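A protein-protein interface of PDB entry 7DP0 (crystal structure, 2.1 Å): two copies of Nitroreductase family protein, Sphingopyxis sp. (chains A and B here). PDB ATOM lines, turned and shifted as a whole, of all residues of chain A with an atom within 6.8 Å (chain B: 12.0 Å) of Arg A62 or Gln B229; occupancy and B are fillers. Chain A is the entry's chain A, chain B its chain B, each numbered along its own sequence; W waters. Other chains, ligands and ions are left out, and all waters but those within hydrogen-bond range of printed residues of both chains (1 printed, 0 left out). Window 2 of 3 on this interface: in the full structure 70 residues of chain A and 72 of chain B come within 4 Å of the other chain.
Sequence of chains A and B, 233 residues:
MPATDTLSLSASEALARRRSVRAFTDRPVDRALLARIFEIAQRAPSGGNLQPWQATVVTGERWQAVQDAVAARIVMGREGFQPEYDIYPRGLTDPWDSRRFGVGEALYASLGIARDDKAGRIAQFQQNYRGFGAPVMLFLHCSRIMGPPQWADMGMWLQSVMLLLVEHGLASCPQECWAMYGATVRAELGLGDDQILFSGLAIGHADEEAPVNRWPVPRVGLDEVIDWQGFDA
The backbone carbonyl oxygen of Asp B227 sits at hydrogen-bond distance from the backbone NH of Val A57.
O of Gln B229 sits at hydrogen-bond distance from N of Thr A59 (3.0 Å).
The backbone carbonyl oxygen of Leu A189 is in hydrogen-bond range of the side-chain amide nitrogen of Gln B229 (3.0 Å).
The guanidinium group (NH2) of Arg A62 sits at hydrogen-bond distance from the side-chain amide oxygen (OE1) of Gln B229 (3.2 Å).
N of Gln B229 lies within hydrogen-bond range of O of Val A57 (2.8 Å).
The side-chain carboxylate (OE2) of Glu A188 is in salt-bridge range of the guanidinium group (NH1) of Arg A62 (3.3 Å).
Among the printed residues, pairs that only touch across the chains: Val A58 with Gln B229 (3.1 Å), Thr A59 with Gly B230 (3.2 Å), Thr A56 with Asp B227 (3.4 Å), Thr A59 with Phe B231 (3.5 Å), Arg A62 with Gly B230 (3.6 Å), Val A57 with Trp B228 (3.6 Å), Thr A56 with Gln B229 (3.6 Å), Val A57 with Phe B231 (3.7 Å) and Val A57 with Ile B226 (3.7 Å).
Thr A56 touches just these residues of chain B: Asp B227 and Gln B229.
Of the printed residues of chain B, Val A57 touches Ile B226, Asp B227, Trp B228, Gln B229 and Phe B231.
Of chain B, only Gln B229 (3.1 Å) comes within 4 Å of Val A58.
No residue of chain B comes within 4 Å of Gly A60.
Arg A62 touches just these residues of chain B: Gln B229 (3.2 Å) and Gly B230 (3.6 Å).
No residue of chain B comes within 4 Å of Trp A63.
No residue of chain B comes within 4 Å of Ala A65.
No residue of chain B comes within 4 Å of Val A66.
No residue of chain B comes within 4 Å of Glu A188.
Of the printed residues of chain B, Leu A189 touches Gln B229.
No residue of chain B comes within 4 Å of Gly A190.
Val B225 touches none of the printed residues of chain A.
Of the printed residues of chain A, Ile B226 touches Val A57 (3.7 Å).
Printed residues of chain A within 4 Å of Trp B228: Val A57 (3.6 Å).
Gln B229 touches just these residues of chain A: Thr A56, Val A57, Val A58, Thr A59, Arg A62 and Leu A189.
Printed residues of chain A within 4 Å of Gly B230: Thr A59 and Arg A62.
Of the printed residues of chain A, Phe B231 touches Val A57 and Thr A59.
The nearest residue of chain A that does not touch Gln B229 is Glu A188 (4.8 Å).
Of the 17 printed residues of chain A, 6 touch a printed residue of chain B.
Of the 8 printed residues of chain B, 6 touch a printed residue of chain A.
Printed residues of chain B that touch a printed residue of chain A: Ile B226, Asp B227, Trp B228, Gln B229, Gly B230 and Phe B231.
Hydrophobic or aromatic side chains of chain B that line the printed part of chain A: Ile B226 and Phe B231.
No position is printed for both chains.
Water W1 lies within hydrogen-bond range of the side-chain carboxylate (OD2) of Asp B227 and the side-chain hydroxyl (OG1) of Thr A56.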
ATOM      1  N   THR A  56      23.916  28.554 -18.552  1.00  0.00           N
ATOM      2  CA  THR A  56      24.103  27.772 -17.351  1.00  0.00           C
ATOM      3  C   THR A  56      23.063  28.274 -16.347  1.00  0.00           C
ATOM      4  O   THR A  56      23.034  29.456 -16.004  1.00  0.00           O
ATOM      5  CB  THR A  56      25.542  27.906 -16.827  1.00  0.00           C
ATOM      6  OG1 THR A  56      26.457  27.526 -17.866  1.00  0.00           O
ATOM      7  CG2 THR A  56      25.771  27.043 -15.602  1.00  0.00           C
ATOM      8  N   VAL A  57      22.157  27.392 -15.940  1.00  0.00           N
ATOM      9  CA  VAL A  57      21.137  27.761 -14.962  1.00  0.00           C
ATOM     10  C   VAL A  57      21.529  27.228 -13.572  1.00  0.00           C
ATOM     11  O   VAL A  57      21.782  26.036 -13.414  1.00  0.00           O
ATOM     12  CB  VAL A  57      19.762  27.219 -15.396  1.00  0.00           C
ATOM     13  CG1 VAL A  57      18.649  27.682 -14.446  1.00  0.00           C
ATOM     14  CG2 VAL A  57      19.458  27.666 -16.817  1.00  0.00           C
ATOM     15  N   VAL A  58      21.557  28.106 -12.569  1.00  0.00           N
ATOM     16  CA  VAL A  58      21.961  27.713 -11.223  1.00  0.00           C
ATOM     17  C   VAL A  58      20.898  28.018 -10.180  1.00  0.00           C
ATOM     18  O   VAL A  58      20.117  28.977 -10.286  1.00  0.00           O
ATOM     19  CB  VAL A  58      23.296  28.404 -10.762  1.00  0.00           C
ATOM     20  CG1 VAL A  58      24.381  28.232 -11.807  1.00  0.00           C
ATOM     21  CG2 VAL A  58      23.093  29.891 -10.465  1.00  0.00           C
ATOM     22  N   THR A  59      20.873  27.175  -9.162  1.00  0.00           N
ATOM     23  CA  THR A  59      20.005  27.393  -8.029  1.00  0.00           C
ATOM     24  C   THR A  59      20.672  26.779  -6.801  1.00  0.00           C
ATOM     25  O   THR A  59      21.766  26.198  -6.892  1.00  0.00           O
ATOM     26  CB  THR A  59      18.612  26.780  -8.245  1.00  0.00           C
ATOM     27  OG1 THR A  59      17.695  27.313  -7.279  1.00  0.00           O
ATOM     28  CG2 THR A  59      18.671  25.254  -8.104  1.00  0.00           C
ATOM     29  N   GLY A  60      20.000  26.909  -5.668  1.00  0.00           N
ATOM     30  CA  GLY A  60      20.486  26.369  -4.416  1.00  0.00           C
ATOM     31  C   GLY A  60      21.924  26.744  -4.108  1.00  0.00           C
ATOM     32  O   GLY A  60      22.343  27.895  -4.299  1.00  0.00           O
ATOM     33  N   GLU A  61      22.691  25.732  -3.711  1.00  0.00           N
ATOM     34  CA  GLU A  61      24.029  25.914  -3.174  1.00  0.00           C
ATOM     35  C   GLU A  61      24.981  26.446  -4.239  1.00  0.00           C
ATOM     36  O   GLU A  61      25.906  27.197  -3.928  1.00  0.00           O
ATOM     37  CB  GLU A  61      24.555  24.600  -2.572  1.00  0.00           C
ATOM     38  CG  GLU A  61      25.274  24.786  -1.229  1.00  0.00           C
ATOM     39  CD  GLU A  61      24.360  25.305  -0.114  1.00  0.00           C
ATOM     40  OE1 GLU A  61      23.412  24.588   0.282  1.00  0.00           O
ATOM     41  OE2 GLU A  61      24.589  26.439   0.368  1.00  0.00           O
ATOM     42  N   ARG A  62      24.758  26.052  -5.488  1.00  0.00           N
ATOM     43  CA  ARG A  62      25.576  26.534  -6.606  1.00  0.00           C
ATOM     44  C   ARG A  62      25.353  28.023  -6.852  1.00  0.00           C
ATOM     45  O   ARG A  62      26.303  28.794  -7.033  1.00  0.00           O
ATOM     46  CB  ARG A  62      25.246  25.728  -7.862  1.00  0.00           C
ATOM     47  CG  ARG A  62      25.646  24.243  -7.744  1.00  0.00           C
ATOM     48  CD  ARG A  62      27.146  24.141  -7.529  1.00  0.00           C
ATOM     49  NE  ARG A  62      27.841  24.781  -8.641  1.00  0.00           N
ATOM     50  CZ  ARG A  62      29.014  25.391  -8.547  1.00  0.00           C
ATOM     51  NH1 ARG A  62      29.633  25.488  -7.374  1.00  0.00           N
ATOM     52  NH2 ARG A  62      29.550  25.934  -9.630  1.00  0.00           N
ATOM     53  N   TRP A  63      24.086  28.419  -6.830  1.00  0.00           N
ATOM     54  CA  TRP A  63      23.691  29.811  -6.904  1.00  0.00           C
ATOM     55  C   TRP A  63      24.316  30.560  -5.714  1.00  0.00           C
ATOM     56  O   TRP A  63      24.709  31.721  -5.832  1.00  0.00           O
ATOM     57  CB  TRP A  63      22.162  29.915  -6.949  1.00  0.00           C
ATOM     58  CG  TRP A  63      21.530  31.285  -6.946  1.00  0.00           C
ATOM     59  CD1 TRP A  63      20.297  31.597  -6.432  1.00  0.00           C
ATOM     60  CD2 TRP A  63      22.067  32.515  -7.471  1.00  0.00           C
ATOM     61  NE1 TRP A  63      20.038  32.932  -6.602  1.00  0.00           N
ATOM     62  CE2 TRP A  63      21.105  33.520  -7.232  1.00  0.00           C
ATOM     63  CE3 TRP A  63      23.267  32.868  -8.109  1.00  0.00           C
ATOM     64  CZ2 TRP A  63      21.304  34.852  -7.608  1.00  0.00           C
ATOM     65  CZ3 TRP A  63      23.460  34.186  -8.485  1.00  0.00           C
ATOM     66  CH2 TRP A  63      22.485  35.165  -8.225  1.00  0.00           C
ATOM     67  N   GLN A  64      24.409  29.887  -4.570  1.00  0.00           N
ATOM     68  CA  GLN A  64      24.976  30.503  -3.388  1.00  0.00           C
ATOM     69  C   GLN A  64      26.496  30.679  -3.540  1.00  0.00           C
ATOM     70  O   GLN A  64      27.068  31.692  -3.117  1.00  0.00           O
ATOM     71  CB  GLN A  64      24.656  29.641  -2.156  1.00  0.00           C
ATOM     72  CG  GLN A  64      24.937  30.314  -0.853  1.00  0.00           C
ATOM     73  CD  GLN A  64      24.236  31.654  -0.742  1.00  0.00           C
ATOM     74  OE1 GLN A  64      24.831  32.698  -1.013  1.00  0.00           O
ATOM     75  NE2 GLN A  64      22.973  31.634  -0.332  1.00  0.00           N
ATOM     76  N   ALA A  65      27.145  29.710  -4.182  1.00  0.00           N
ATOM     77  CA  ALA A  65      28.586  29.791  -4.401  1.00  0.00           C
ATOM     78  C   ALA A  65      28.964  30.957  -5.305  1.00  0.00           C
ATOM     79  O   ALA A  65      29.889  31.712  -4.992  1.00  0.00           O
ATOM     80  CB  ALA A  65      29.111  28.493  -4.976  1.00  0.00           C
ATOM     81  N   VAL A  66      28.234  31.120  -6.407  1.00  0.00           N
ATOM     82  CA  VAL A  66      28.483  32.222  -7.330  1.00  0.00           C
ATOM     83  C   VAL A  66      28.366  33.548  -6.585  1.00  0.00           C
ATOM     84  O   VAL A  66      29.270  34.388  -6.671  1.00  0.00           O
ATOM     85  CB  VAL A  66      27.498  32.217  -8.526  1.00  0.00           C
ATOM     86  CG1 VAL A  66      27.678  33.465  -9.406  1.00  0.00           C
ATOM     87  CG2 VAL A  66      27.653  30.945  -9.355  1.00  0.00           C
ATOM     88  N   GLN A  67      27.282  33.719  -5.826  1.00  0.00           N
ATOM     89  CA  GLN A  67      27.097  34.947  -5.061  1.00  0.00           C
ATOM     90  C   GLN A  67      28.294  35.204  -4.152  1.00  0.00           C
ATOM     91  O   GLN A  67      28.803  36.319  -4.125  1.00  0.00           O
ATOM     92  CB  GLN A  67      25.802  34.907  -4.223  1.00  0.00           C
ATOM     93  CG  GLN A  67      24.515  34.805  -5.041  1.00  0.00           C
ATOM     94  CD  GLN A  67      23.258  34.776  -4.174  1.00  0.00           C
ATOM     95  OE1 GLN A  67      23.083  35.603  -3.293  1.00  0.00           O
ATOM     96  NE2 GLN A  67      22.406  33.778  -4.396  1.00  0.00           N
ATOM     97  N   ALA A 187      34.697  31.075 -13.713  1.00  0.00           N
ATOM     98  CA  ALA A 187      35.479  30.102 -12.930  1.00  0.00           C
ATOM     99  C   ALA A 187      34.584  29.313 -11.977  1.00  0.00           C
ATOM    100  O   ALA A 187      34.748  28.100 -11.811  1.00  0.00           O
ATOM    101  CB  ALA A 187      36.600  30.792 -12.143  1.00  0.00           C
ATOM    102  N   GLU A 188      33.630  30.007 -11.361  1.00  0.00           N
ATOM    103  CA  GLU A 188      32.752  29.388 -10.385  1.00  0.00           C
ATOM    104  C   GLU A 188      31.811  28.402 -11.064  1.00  0.00           C
ATOM    105  O   GLU A 188      31.462  27.363 -10.508  1.00  0.00           O
ATOM    106  CB  GLU A 188      31.951  30.447  -9.627  1.00  0.00           C
ATOM    107  CG  GLU A 188      31.213  29.885  -8.450  1.00  0.00           C
ATOM    108  CD  GLU A 188      32.145  29.131  -7.522  1.00  0.00           C
ATOM    109  OE1 GLU A 188      33.274  29.626  -7.269  1.00  0.00           O
ATOM    110  OE2 GLU A 188      31.762  28.029  -7.075  1.00  0.00           O
ATOM    111  N   LEU A 189      31.389  28.735 -12.271  1.00  0.00           N
ATOM    112  CA  LEU A 189      30.470  27.870 -12.993  1.00  0.00           C
ATOM    113  C   LEU A 189      31.196  26.675 -13.634  1.00  0.00           C
ATOM    114  O   LEU A 189      30.569  25.685 -14.028  1.00  0.00           O
ATOM    115  CB  LEU A 189      29.722  28.680 -14.052  1.00  0.00           C
ATOM    116  CG  LEU A 189      28.811  29.834 -13.619  1.00  0.00           C
ATOM    117  CD1 LEU A 189      28.281  30.520 -14.865  1.00  0.00           C
ATOM    118  CD2 LEU A 189      27.642  29.362 -12.776  1.00  0.00           C
ATOM    119  N   GLY A 190      32.521  26.766 -13.712  1.00  0.00           N
ATOM    120  CA  GLY A 190      33.327  25.750 -14.366  1.00  0.00           C
ATOM    121  C   GLY A 190      33.402  25.973 -15.861  1.00  0.00           C
ATOM    122  O   GLY A 190      33.654  25.045 -16.615  1.00  0.00           O
ATOM    123  N   LEU A 191      33.186  27.208 -16.307  1.00  0.00           N
ATOM    124  CA  LEU A 191      33.274  27.493 -17.735  1.00  0.00           C
ATOM    125  C   LEU A 191      34.719  27.851 -18.120  1.00  0.00           C
ATOM    126  O   LEU A 191      35.407  28.538 -17.375  1.00  0.00           O
ATOM    127  CB  LEU A 191      32.309  28.621 -18.127  1.00  0.00           C
ATOM    128  CG  LEU A 191      30.807  28.355 -17.981  1.00  0.00           C
ATOM    129  CD1 LEU A 191      30.022  29.650 -18.181  1.00  0.00           C
ATOM    130  CD2 LEU A 191      30.308  27.293 -18.967  1.00  0.00           C
ATOM    131  N   LEU B 222      17.737  20.696 -26.105  1.00  0.00           N
ATOM    132  CA  LEU B 222      18.189  21.443 -24.929  1.00  0.00           C
ATOM    133  C   LEU B 222      19.470  20.866 -24.309  1.00  0.00           C
ATOM    134  O   LEU B 222      20.165  21.547 -23.561  1.00  0.00           O
ATOM    135  CB  LEU B 222      17.089  21.478 -23.878  1.00  0.00           C
ATOM    136  CG  LEU B 222      15.930  22.427 -24.168  1.00  0.00           C
ATOM    137  CD1 LEU B 222      15.083  22.634 -22.903  1.00  0.00           C
ATOM    138  CD2 LEU B 222      16.469  23.759 -24.707  1.00  0.00           C
ATOM    139  N   VAL B 225      22.101  22.951 -25.098  1.00  0.00           N
ATOM    140  CA  VAL B 225      21.870  24.362 -24.793  1.00  0.00           C
ATOM    141  C   VAL B 225      21.997  24.741 -23.315  1.00  0.00           C
ATOM    142  O   VAL B 225      22.645  25.729 -22.968  1.00  0.00           O
ATOM    143  CB  VAL B 225      20.471  24.792 -25.248  1.00  0.00           C
ATOM    144  CG1 VAL B 225      20.315  26.294 -25.057  1.00  0.00           C
ATOM    145  CG2 VAL B 225      20.216  24.381 -26.708  1.00  0.00           C
ATOM    146  N   ILE B 226      21.358  23.955 -22.456  1.00  0.00           N
ATOM    147  CA  ILE B 226      21.204  24.320 -21.061  1.00  0.00           C
ATOM    148  C   ILE B 226      22.023  23.368 -20.188  1.00  0.00           C
ATOM    149  O   ILE B 226      21.913  22.148 -20.325  1.00  0.00           O
ATOM    150  CB  ILE B 226      19.714  24.260 -20.612  1.00  0.00           C
ATOM    151  CG1 ILE B 226      18.801  24.958 -21.627  1.00  0.00           C
ATOM    152  CG2 ILE B 226      19.538  24.838 -19.197  1.00  0.00           C
ATOM    153  CD1 ILE B 226      18.787  26.479 -21.519  1.00  0.00           C
ATOM    154  N   ASP B 227      22.847  23.945 -19.316  1.00  0.00           N
ATOM    155  CA  ASP B 227      23.495  23.226 -18.215  1.00  0.00           C
ATOM    156  C   ASP B 227      22.794  23.571 -16.907  1.00  0.00           C
ATOM    157  O   ASP B 227      22.664  24.744 -16.569  1.00  0.00           O
ATOM    158  CB  ASP B 227      24.974  23.600 -18.108  1.00  0.00           C
ATOM    159  CG  ASP B 227      25.747  22.693 -17.144  1.00  0.00           C
ATOM    160  OD1 ASP B 227      25.135  21.803 -16.512  1.00  0.00           O
ATOM    161  OD2 ASP B 227      26.962  22.929 -16.969  1.00  0.00           O
ATOM    162  N   TRP B 228      22.369  22.553 -16.166  1.00  0.00           N
ATOM    163  CA  TRP B 228      21.702  22.751 -14.882  1.00  0.00           C
ATOM    164  C   TRP B 228      22.646  22.504 -13.709  1.00  0.00           C
ATOM    165  O   TRP B 228      23.257  21.434 -13.626  1.00  0.00           O
ATOM    166  CB  TRP B 228      20.495  21.807 -14.763  1.00  0.00           C
ATOM    167  CG  TRP B 228      19.616  21.792 -15.974  1.00  0.00           C
ATOM    168  CD1 TRP B 228      19.792  21.046 -17.106  1.00  0.00           C
ATOM    169  CD2 TRP B 228      18.417  22.552 -16.176  1.00  0.00           C
ATOM    170  NE1 TRP B 228      18.775  21.299 -18.004  1.00  0.00           N
ATOM    171  CE2 TRP B 228      17.921  22.220 -17.455  1.00  0.00           C
ATOM    172  CE3 TRP B 228      17.713  23.482 -15.402  1.00  0.00           C
ATOM    173  CZ2 TRP B 228      16.757  22.781 -17.969  1.00  0.00           C
ATOM    174  CZ3 TRP B 228      16.552  24.033 -15.917  1.00  0.00           C
ATOM    175  CH2 TRP B 228      16.088  23.680 -17.185  1.00  0.00           C
ATOM    176  N   GLN B 229      22.736  23.469 -12.792  1.00  0.00           N
ATOM    177  CA  GLN B 229      23.575  23.325 -11.604  1.00  0.00           C
ATOM    178  C   GLN B 229      22.798  23.677 -10.344  1.00  0.00           C
ATOM    179  O   GLN B 229      22.146  24.720 -10.279  1.00  0.00           O
ATOM    180  CB  GLN B 229      24.836  24.200 -11.701  1.00  0.00           C
ATOM    181  CG  GLN B 229      25.711  23.904 -12.919  1.00  0.00           C
ATOM    182  CD  GLN B 229      27.034  24.658 -12.893  1.00  0.00           C
ATOM    183  OE1 GLN B 229      27.355  25.316 -11.908  1.00  0.00           O
ATOM    184  NE2 GLN B 229      27.812  24.551 -13.970  1.00  0.00           N
ATOM    185  N   GLY B 230      22.834  22.780  -9.362  1.00  0.00           N
ATOM    186  CA  GLY B 230      22.234  23.051  -8.068  1.00  0.00           C
ATOM    187  C   GLY B 230      20.828  22.526  -7.843  1.00  0.00           C
ATOM    188  O   GLY B 230      20.236  22.781  -6.800  1.00  0.00           O
ATOM    189  N   PHE B 231      20.277  21.799  -8.805  1.00  0.00           N
ATOM    190  CA  PHE B 231      18.908  21.315  -8.658  1.00  0.00           C
ATOM    191  C   PHE B 231      18.832  19.925  -8.043  1.00  0.00           C
ATOM    192  O   PHE B 231      19.689  19.089  -8.301  1.00  0.00           O
ATOM    193  CB  PHE B 231      18.206  21.321 -10.004  1.00  0.00           C
ATOM    194  CG  PHE B 231      18.009  22.692 -10.563  1.00  0.00           C
ATOM    195  CD1 PHE B 231      16.795  23.345 -10.404  1.00  0.00           C
ATOM    196  CD2 PHE B 231      19.031  23.339 -11.240  1.00  0.00           C
ATOM    197  CE1 PHE B 231      16.603  24.617 -10.925  1.00  0.00           C
ATOM    198  CE2 PHE B 231      18.837  24.617 -11.760  1.00  0.00           C
ATOM    199  CZ  PHE B 231      17.631  25.252 -11.595  1.00  0.00           C
HETATM  200  O   HOH W   1      28.106  25.332 -17.383  1.00  0.00           O
